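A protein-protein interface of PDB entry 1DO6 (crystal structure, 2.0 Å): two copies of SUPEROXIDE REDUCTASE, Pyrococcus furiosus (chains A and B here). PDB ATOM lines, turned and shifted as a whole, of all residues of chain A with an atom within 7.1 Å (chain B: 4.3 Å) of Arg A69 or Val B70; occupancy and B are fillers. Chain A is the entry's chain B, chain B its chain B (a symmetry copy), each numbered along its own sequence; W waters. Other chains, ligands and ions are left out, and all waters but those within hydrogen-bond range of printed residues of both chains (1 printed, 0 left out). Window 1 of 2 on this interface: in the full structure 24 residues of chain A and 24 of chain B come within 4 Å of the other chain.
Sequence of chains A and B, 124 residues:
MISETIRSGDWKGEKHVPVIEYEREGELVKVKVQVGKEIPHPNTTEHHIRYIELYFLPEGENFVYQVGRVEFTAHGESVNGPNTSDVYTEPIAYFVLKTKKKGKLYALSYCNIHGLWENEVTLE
N of Glu B71 lies within hydrogen-bond range of O of Arg A69, 2.8 Å away. The backbone NH (N) of Glu A71 sits at hydrogen-bond distance from the backbone carbonyl oxygen (O) of Arg B69 (2.8 Å).
The backbone carbonyl oxygen (O) of Ile A52 is in hydrogen-bond range of the backbone NH (N) of Val A70 (2.9 Å). The side-chain carboxylate (OE2) of Glu A53 is in salt-bridge range of the guanidinium group (NH1) of Arg A69, at 2.8 Å. The backbone carbonyl oxygen (O) of Gly A68 is in hydrogen-bond range of the backbone NH (N) of Leu A54. The side-chain carboxylate of Glu A71 is in salt-bridge range of the guanidinium group of Arg A69. O of Ile B52 sits at hydrogen-bond distance from N of Val B70, 2.9 Å away. The side-chain carboxylate of Glu B71 is in salt-bridge range of the guanidinium group of Arg B69, 2.8 Å away.
Glu B71 touches Gly A68 (O to CA, 3.3 Å). O of Arg B69 touches O of Arg A69, at 3.8 Å. O of Arg A69 touches CA of Val B70 (3.4 Å). Val A70 touches Arg B69 (CA to O, 3.4 Å).
Gln A66 touches none of the printed residues of chain B. Of the printed residues of chain B, Gly A68 touches Glu B71. Arg A69 touches three residues of chain B. Of the printed residues of chain B, Glu A71 touches Arg B69 (2.8 Å). Of chain A, only Arg A69 comes within 4 Å of Val B70. The nearest printed residue of chain B that does not touch Gly A68 is Phe B72 (5.0 Å).
Hydrophobic or aromatic side chains of chain A within 4 Å of the printed part of chain B: Val A70. Printed residues of chain B that touch a printed residue of chain A: Arg B69, Val B70 and Glu B71. Hydrophobic or aromatic side chains of chain B that line the printed part of chain A: Val B70. Among the printed residues, 6 pairs touch across the chains.
Arg A69 touches its own counterpart, Arg B69. Arg A69 touches Val B70, and with the chains exchanged Val A70 touches Arg B69. Arg A69 touches Glu B71, and with the chains exchanged Glu A71 touches Arg B69. Positions printed for both chains: 51, 52, 69, 70, 71, 93 and 95. Of the 6 pairs that touch across the chains among the printed residues, 5 have their exchanged pair printed and touching as well.
Water W1 lies within hydrogen-bond range of the side-chain amide nitrogen (NE2) of Gln A66 (2.9 Å) and the side-chain carboxylate (OE2) of Glu B71 (2.9 Å).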
ATOM      1  N   ARG A  50      28.107  -1.162  -4.449  1.00  0.00           N
ATOM      2  CA  ARG A  50      28.504  -2.330  -3.674  1.00  0.00           C
ATOM      3  C   ARG A  50      28.081  -3.691  -4.272  1.00  0.00           C
ATOM      4  O   ARG A  50      28.859  -4.647  -4.260  1.00  0.00           O
ATOM      5  CB  ARG A  50      27.947  -2.231  -2.258  1.00  0.00           C
ATOM      6  CG  ARG A  50      28.514  -1.087  -1.402  1.00  0.00           C
ATOM      7  CD  ARG A  50      29.853  -1.483  -0.775  1.00  0.00           C
ATOM      8  NE  ARG A  50      30.319  -0.531   0.231  1.00  0.00           N
ATOM      9  CZ  ARG A  50      29.810  -0.403   1.454  1.00  0.00           C
ATOM     10  NH1 ARG A  50      28.793  -1.174   1.850  1.00  0.00           N
ATOM     11  NH2 ARG A  50      30.319   0.492   2.298  1.00  0.00           N
ATOM     12  N   TYR A  51      26.862  -3.779  -4.794  1.00  0.00           N
ATOM     13  CA  TYR A  51      26.399  -5.061  -5.342  1.00  0.00           C
ATOM     14  C   TYR A  51      25.150  -4.925  -6.186  1.00  0.00           C
ATOM     15  O   TYR A  51      24.511  -3.875  -6.178  1.00  0.00           O
ATOM     16  CB  TYR A  51      26.097  -6.021  -4.190  1.00  0.00           C
ATOM     17  CG  TYR A  51      24.948  -5.570  -3.321  1.00  0.00           C
ATOM     18  CD1 TYR A  51      23.615  -5.676  -3.758  1.00  0.00           C
ATOM     19  CD2 TYR A  51      25.181  -5.044  -2.062  1.00  0.00           C
ATOM     20  CE1 TYR A  51      22.550  -5.265  -2.944  1.00  0.00           C
ATOM     21  CE2 TYR A  51      24.130  -4.627  -1.241  1.00  0.00           C
ATOM     22  CZ  TYR A  51      22.815  -4.748  -1.691  1.00  0.00           C
ATOM     23  OH  TYR A  51      21.785  -4.362  -0.855  1.00  0.00           O
ATOM     24  N   ILE A  52      24.823  -5.997  -6.912  1.00  0.00           N
ATOM     25  CA  ILE A  52      23.622  -6.070  -7.737  1.00  0.00           C
ATOM     26  C   ILE A  52      22.984  -7.452  -7.461  1.00  0.00           C
ATOM     27  O   ILE A  52      23.673  -8.477  -7.472  1.00  0.00           O
ATOM     28  CB  ILE A  52      23.945  -5.978  -9.266  1.00  0.00           C
ATOM     29  CG1 ILE A  52      24.251  -4.534  -9.672  1.00  0.00           C
ATOM     30  CG2 ILE A  52      22.754  -6.479 -10.087  1.00  0.00           C
ATOM     31  CD1 ILE A  52      24.772  -4.391 -11.119  1.00  0.00           C
ATOM     32  N   GLU A  53      21.682  -7.467  -7.203  1.00  0.00           N
ATOM     33  CA  GLU A  53      20.947  -8.710  -6.943  1.00  0.00           C
ATOM     34  C   GLU A  53      19.866  -8.844  -7.987  1.00  0.00           C
ATOM     35  O   GLU A  53      19.268  -7.844  -8.401  1.00  0.00           O
ATOM     36  CB  GLU A  53      20.275  -8.682  -5.577  1.00  0.00           C
ATOM     37  CG  GLU A  53      21.244  -8.830  -4.454  1.00  0.00           C
ATOM     38  CD  GLU A  53      20.591  -8.668  -3.104  1.00  0.00           C
ATOM     39  OE1 GLU A  53      19.457  -8.135  -3.021  1.00  0.00           O
ATOM     40  OE2 GLU A  53      21.231  -9.086  -2.119  1.00  0.00           O
ATOM     41  N   LEU A  54      19.603 -10.079  -8.398  1.00  0.00           N
ATOM     42  CA  LEU A  54      18.582 -10.346  -9.400  1.00  0.00           C
ATOM     43  C   LEU A  54      17.533 -11.290  -8.806  1.00  0.00           C
ATOM     44  O   LEU A  54      17.877 -12.288  -8.170  1.00  0.00           O
ATOM     45  CB  LEU A  54      19.225 -10.976 -10.641  1.00  0.00           C
ATOM     46  CG  LEU A  54      18.266 -11.222 -11.799  1.00  0.00           C
ATOM     47  CD1 LEU A  54      17.839  -9.888 -12.399  1.00  0.00           C
ATOM     48  CD2 LEU A  54      18.904 -12.103 -12.839  1.00  0.00           C
ATOM     49  N   TYR A  55      16.262 -10.947  -9.012  1.00  0.00           N
ATOM     50  CA  TYR A  55      15.142 -11.731  -8.528  1.00  0.00           C
ATOM     51  C   TYR A  55      14.266 -12.097  -9.708  1.00  0.00           C
ATOM     52  O   TYR A  55      14.298 -11.434 -10.747  1.00  0.00           O
ATOM     53  CB  TYR A  55      14.322 -10.931  -7.530  1.00  0.00           C
ATOM     54  CG  TYR A  55      15.087 -10.591  -6.282  1.00  0.00           C
ATOM     55  CD1 TYR A  55      15.944  -9.482  -6.251  1.00  0.00           C
ATOM     56  CD2 TYR A  55      14.972 -11.380  -5.141  1.00  0.00           C
ATOM     57  CE1 TYR A  55      16.666  -9.175  -5.107  1.00  0.00           C
ATOM     58  CE2 TYR A  55      15.690 -11.086  -3.977  1.00  0.00           C
ATOM     59  CZ  TYR A  55      16.541  -9.977  -3.974  1.00  0.00           C
ATOM     60  OH  TYR A  55      17.286  -9.690  -2.864  1.00  0.00           O
ATOM     61  N   GLN A  66      15.195 -15.374  -5.395  1.00  0.00           N
ATOM     62  CA  GLN A  66      16.421 -14.626  -5.614  1.00  0.00           C
ATOM     63  C   GLN A  66      17.206 -15.532  -6.575  1.00  0.00           C
ATOM     64  O   GLN A  66      17.403 -16.725  -6.291  1.00  0.00           O
ATOM     65  CB  GLN A  66      17.205 -14.459  -4.321  1.00  0.00           C
ATOM     66  CG  GLN A  66      18.538 -13.708  -4.526  1.00  0.00           C
ATOM     67  CD  GLN A  66      19.154 -13.368  -3.196  1.00  0.00           C
ATOM     68  OE1 GLN A  66      19.049 -12.229  -2.704  1.00  0.00           O
ATOM     69  NE2 GLN A  66      19.782 -14.354  -2.585  1.00  0.00           N
ATOM     70  N   VAL A  67      17.614 -14.986  -7.716  1.00  0.00           N
ATOM     71  CA  VAL A  67      18.357 -15.725  -8.727  1.00  0.00           C
ATOM     72  C   VAL A  67      19.871 -15.680  -8.460  1.00  0.00           C
ATOM     73  O   VAL A  67      20.597 -16.671  -8.630  1.00  0.00           O
ATOM     74  CB  VAL A  67      18.078 -15.122 -10.121  1.00  0.00           C
ATOM     75  CG1 VAL A  67      18.989 -15.740 -11.174  1.00  0.00           C
ATOM     76  CG2 VAL A  67      16.627 -15.331 -10.472  1.00  0.00           C
ATOM     77  N   GLY A  68      20.355 -14.522  -8.028  1.00  0.00           N
ATOM     78  CA  GLY A  68      21.772 -14.428  -7.777  1.00  0.00           C
ATOM     79  C   GLY A  68      22.121 -13.086  -7.180  1.00  0.00           C
ATOM     80  O   GLY A  68      21.303 -12.149  -7.133  1.00  0.00           O
ATOM     81  N   ARG A  69      23.361 -13.000  -6.730  1.00  0.00           N
ATOM     82  CA  ARG A  69      23.860 -11.785  -6.103  1.00  0.00           C
ATOM     83  C   ARG A  69      25.327 -11.639  -6.506  1.00  0.00           C
ATOM     84  O   ARG A  69      26.076 -12.617  -6.479  1.00  0.00           O
ATOM     85  CB  ARG A  69      23.729 -11.939  -4.592  1.00  0.00           C
ATOM     86  CG  ARG A  69      24.246 -10.801  -3.784  1.00  0.00           C
ATOM     87  CD  ARG A  69      24.040 -11.086  -2.309  1.00  0.00           C
ATOM     88  NE  ARG A  69      25.062 -10.384  -1.550  1.00  0.00           N
ATOM     89  CZ  ARG A  69      24.945  -9.111  -1.209  1.00  0.00           C
ATOM     90  NH1 ARG A  69      23.862  -8.449  -1.564  1.00  0.00           N
ATOM     91  NH2 ARG A  69      25.898  -8.499  -0.532  1.00  0.00           N
ATOM     92  N   VAL A  70      25.724 -10.434  -6.916  1.00  0.00           N
ATOM     93  CA  VAL A  70      27.116 -10.186  -7.294  1.00  0.00           C
ATOM     94  C   VAL A  70      27.635  -9.027  -6.470  1.00  0.00           C
ATOM     95  O   VAL A  70      26.998  -7.965  -6.429  1.00  0.00           O
ATOM     96  CB  VAL A  70      27.272  -9.814  -8.776  1.00  0.00           C
ATOM     97  CG1 VAL A  70      28.779  -9.677  -9.115  1.00  0.00           C
ATOM     98  CG2 VAL A  70      26.646 -10.890  -9.662  1.00  0.00           C
ATOM     99  N   GLU A  71      28.755  -9.246  -5.786  1.00  0.00           N
ATOM    100  CA  GLU A  71      29.367  -8.198  -4.968  1.00  0.00           C
ATOM    101  C   GLU A  71      30.616  -7.678  -5.672  1.00  0.00           C
ATOM    102  O   GLU A  71      31.431  -8.473  -6.152  1.00  0.00           O
ATOM    103  CB  GLU A  71      29.735  -8.743  -3.594  1.00  0.00           C
ATOM    104  CG  GLU A  71      28.528  -9.130  -2.774  1.00  0.00           C
ATOM    105  CD  GLU A  71      28.895  -9.779  -1.449  1.00  0.00           C
ATOM    106  OE1 GLU A  71      27.980 -10.288  -0.770  1.00  0.00           O
ATOM    107  OE2 GLU A  71      30.090  -9.785  -1.085  1.00  0.00           O
ATOM    108  N   ALA A  93      27.044  -7.022 -13.843  1.00  0.00           N
ATOM    109  CA  ALA A  93      26.694  -8.370 -13.398  1.00  0.00           C
ATOM    110  C   ALA A  93      26.096  -9.220 -14.520  1.00  0.00           C
ATOM    111  O   ALA A  93      25.287  -8.746 -15.317  1.00  0.00           O
ATOM    112  CB  ALA A  93      25.708  -8.288 -12.228  1.00  0.00           C
ATOM    113  N   TYR A  94      26.510 -10.484 -14.561  1.00  0.00           N
ATOM    114  CA  TYR A  94      26.033 -11.449 -15.542  1.00  0.00           C
ATOM    115  C   TYR A  94      25.457 -12.643 -14.806  1.00  0.00           C
ATOM    116  O   TYR A  94      26.064 -13.152 -13.863  1.00  0.00           O
ATOM    117  CB  TYR A  94      27.169 -11.973 -16.395  1.00  0.00           C
ATOM    118  CG  TYR A  94      27.540 -11.079 -17.531  1.00  0.00           C
ATOM    119  CD1 TYR A  94      28.221  -9.876 -17.303  1.00  0.00           C
ATOM    120  CD2 TYR A  94      27.236 -11.435 -18.844  1.00  0.00           C
ATOM    121  CE1 TYR A  94      28.591  -9.041 -18.368  1.00  0.00           C
ATOM    122  CE2 TYR A  94      27.601 -10.609 -19.919  1.00  0.00           C
ATOM    123  CZ  TYR A  94      28.276  -9.415 -19.674  1.00  0.00           C
ATOM    124  OH  TYR A  94      28.622  -8.597 -20.733  1.00  0.00           O
ATOM    125  N   PHE A  95      24.292 -13.097 -15.232  1.00  0.00           N
ATOM    126  CA  PHE A  95      23.707 -14.267 -14.600  1.00  0.00           C
ATOM    127  C   PHE A  95      23.208 -15.220 -15.685  1.00  0.00           C
ATOM    128  O   PHE A  95      22.632 -14.790 -16.687  1.00  0.00           O
ATOM    129  CB  PHE A  95      22.523 -13.891 -13.698  1.00  0.00           C
ATOM    130  CG  PHE A  95      22.854 -12.921 -12.590  1.00  0.00           C
ATOM    131  CD1 PHE A  95      22.644 -11.550 -12.757  1.00  0.00           C
ATOM    132  CD2 PHE A  95      23.311 -13.382 -11.356  1.00  0.00           C
ATOM    133  CE1 PHE A  95      22.875 -10.654 -11.706  1.00  0.00           C
ATOM    134  CE2 PHE A  95      23.547 -12.497 -10.298  1.00  0.00           C
ATOM    135  CZ  PHE A  95      23.325 -11.132 -10.471  1.00  0.00           C
ATOM    136  N   LEU A 108      18.160  -5.269  -7.965  1.00  0.00           N
ATOM    137  CA  LEU A 108      18.298  -4.404  -6.806  1.00  0.00           C
ATOM    138  C   LEU A 108      19.781  -4.022  -6.728  1.00  0.00           C
ATOM    139  O   LEU A 108      20.660  -4.899  -6.761  1.00  0.00           O
ATOM    140  CB  LEU A 108      17.868  -5.152  -5.550  1.00  0.00           C
ATOM    141  CG  LEU A 108      17.438  -4.330  -4.346  1.00  0.00           C
ATOM    142  CD1 LEU A 108      16.345  -3.344  -4.754  1.00  0.00           C
ATOM    143  CD2 LEU A 108      16.949  -5.264  -3.257  1.00  0.00           C
ATOM    144  N   TYR B  51      28.674 -20.707  -4.622  1.00  0.00           N
ATOM    145  CA  TYR B  51      29.245 -19.424  -5.051  1.00  0.00           C
ATOM    146  C   TYR B  51      30.648 -19.558  -5.604  1.00  0.00           C
ATOM    147  O   TYR B  51      31.271 -20.608  -5.459  1.00  0.00           O
ATOM    148  CB  TYR B  51      29.289 -18.468  -3.859  1.00  0.00           C
ATOM    149  CG  TYR B  51      30.220 -18.923  -2.762  1.00  0.00           C
ATOM    150  CD1 TYR B  51      31.617 -18.816  -2.896  1.00  0.00           C
ATOM    151  CD2 TYR B  51      29.718 -19.452  -1.585  1.00  0.00           C
ATOM    152  CE1 TYR B  51      32.478 -19.230  -1.871  1.00  0.00           C
ATOM    153  CE2 TYR B  51      30.565 -19.872  -0.556  1.00  0.00           C
ATOM    154  CZ  TYR B  51      31.947 -19.751  -0.708  1.00  0.00           C
ATOM    155  OH  TYR B  51      32.769 -20.140   0.332  1.00  0.00           O
ATOM    156  N   ILE B  52      31.126 -18.484  -6.236  1.00  0.00           N
ATOM    157  CA  ILE B  52      32.477 -18.408  -6.780  1.00  0.00           C
ATOM    158  C   ILE B  52      33.040 -17.027  -6.367  1.00  0.00           C
ATOM    159  O   ILE B  52      32.369 -16.002  -6.524  1.00  0.00           O
ATOM    160  CB  ILE B  52      32.496 -18.495  -8.343  1.00  0.00           C
ATOM    161  CG1 ILE B  52      32.286 -19.938  -8.810  1.00  0.00           C
ATOM    162  CG2 ILE B  52      33.838 -17.991  -8.882  1.00  0.00           C
ATOM    163  CD1 ILE B  52      32.094 -20.075 -10.337  1.00  0.00           C
ATOM    164  N   ARG B  69      32.510 -11.481  -5.717  1.00  0.00           N
ATOM    165  CA  ARG B  69      31.886 -12.699  -5.218  1.00  0.00           C
ATOM    166  C   ARG B  69      30.543 -12.843  -5.932  1.00  0.00           C
ATOM    167  O   ARG B  69      29.806 -11.864  -6.066  1.00  0.00           O
ATOM    168  CB  ARG B  69      31.685 -12.549  -3.714  1.00  0.00           C
ATOM    169  CG  ARG B  69      31.004 -13.690  -3.042  1.00  0.00           C
ATOM    170  CD  ARG B  69      30.883 -13.411  -1.557  1.00  0.00           C
ATOM    171  NE  ARG B  69      29.721 -14.114  -1.042  1.00  0.00           N
ATOM    172  CZ  ARG B  69      29.761 -15.388  -0.687  1.00  0.00           C
ATOM    173  NH1 ARG B  69      30.895 -16.049  -0.800  1.00  0.00           N
ATOM    174  NH2 ARG B  69      28.683 -16.002  -0.237  1.00  0.00           N
ATOM    175  N   VAL B  70      30.245 -14.046  -6.423  1.00  0.00           N
ATOM    176  CA  VAL B  70      28.969 -14.292  -7.096  1.00  0.00           C
ATOM    177  C   VAL B  70      28.284 -15.454  -6.409  1.00  0.00           C
ATOM    178  O   VAL B  70      28.897 -16.517  -6.234  1.00  0.00           O
ATOM    179  CB  VAL B  70      29.141 -14.659  -8.578  1.00  0.00           C
ATOM    180  CG1 VAL B  70      27.745 -14.795  -9.238  1.00  0.00           C
ATOM    181  CG2 VAL B  70      29.945 -13.581  -9.302  1.00  0.00           C
ATOM    182  N   GLU B  71      27.041 -15.237  -5.986  1.00  0.00           N
ATOM    183  CA  GLU B  71      26.266 -16.287  -5.324  1.00  0.00           C
ATOM    184  C   GLU B  71      25.201 -16.804  -6.285  1.00  0.00           C
ATOM    185  O   GLU B  71      24.510 -16.007  -6.929  1.00  0.00           O
ATOM    186  CB  GLU B  71      25.607 -15.747  -4.062  1.00  0.00           C
ATOM    187  CG  GLU B  71      26.605 -15.362  -2.997  1.00  0.00           C
ATOM    188  CD  GLU B  71      25.958 -14.718  -1.781  1.00  0.00           C
ATOM    189  OE1 GLU B  71      26.703 -14.212  -0.918  1.00  0.00           O
ATOM    190  OE2 GLU B  71      24.713 -14.713  -1.688  1.00  0.00           O
ATOM    191  N   PHE B  72      25.099 -18.130  -6.396  1.00  0.00           N
ATOM    192  CA  PHE B  72      24.110 -18.791  -7.264  1.00  0.00           C
ATOM    193  C   PHE B  72      23.061 -19.265  -6.240  1.00  0.00           C
ATOM    194  O   PHE B  72      23.296 -20.170  -5.448  1.00  0.00           O
ATOM    195  CB  PHE B  72      24.797 -19.941  -7.997  1.00  0.00           C
ATOM    196  CG  PHE B  72      26.118 -19.549  -8.622  1.00  0.00           C
ATOM    197  CD1 PHE B  72      27.306 -20.146  -8.205  1.00  0.00           C
ATOM    198  CD2 PHE B  72      26.172 -18.571  -9.634  1.00  0.00           C
ATOM    199  CE1 PHE B  72      28.536 -19.784  -8.787  1.00  0.00           C
ATOM    200  CE2 PHE B  72      27.389 -18.202 -10.213  1.00  0.00           C
ATOM    201  CZ  PHE B  72      28.572 -18.811  -9.794  1.00  0.00           C
ATOM    202  N   ALA B  93      30.470 -17.435 -13.482  1.00  0.00           N
ATOM    203  CA  ALA B  93      30.714 -16.089 -12.967  1.00  0.00           C
ATOM    204  C   ALA B  93      31.543 -15.235 -13.929  1.00  0.00           C
ATOM    205  O   ALA B  93      32.506 -15.706 -14.531  1.00  0.00           O
ATOM    206  CB  ALA B  93      31.421 -16.175 -11.611  1.00  0.00           C
ATOM    207  N   PHE B  95      33.457 -11.356 -14.217  1.00  0.00           N
ATOM    208  CA  PHE B  95      33.890 -10.189 -13.469  1.00  0.00           C
ATOM    209  C   PHE B  95      34.612  -9.232 -14.416  1.00  0.00           C
ATOM    210  O   PHE B  95      35.393  -9.659 -15.269  1.00  0.00           O
ATOM    211  CB  PHE B  95      34.849 -10.568 -12.331  1.00  0.00           C
ATOM    212  CG  PHE B  95      34.283 -11.542 -11.325  1.00  0.00           C
ATOM    213  CD1 PHE B  95      34.526 -12.912 -11.447  1.00  0.00           C
ATOM    214  CD2 PHE B  95      33.568 -11.085 -10.219  1.00  0.00           C
ATOM    215  CE1 PHE B  95      34.071 -13.811 -10.475  1.00  0.00           C
ATOM    216  CE2 PHE B  95      33.108 -11.973  -9.241  1.00  0.00           C
ATOM    217  CZ  PHE B  95      33.362 -13.337  -9.366  1.00  0.00           C
HETATM  218  O   HOH W   1      21.995 -14.391  -0.769  1.00  0.00           O
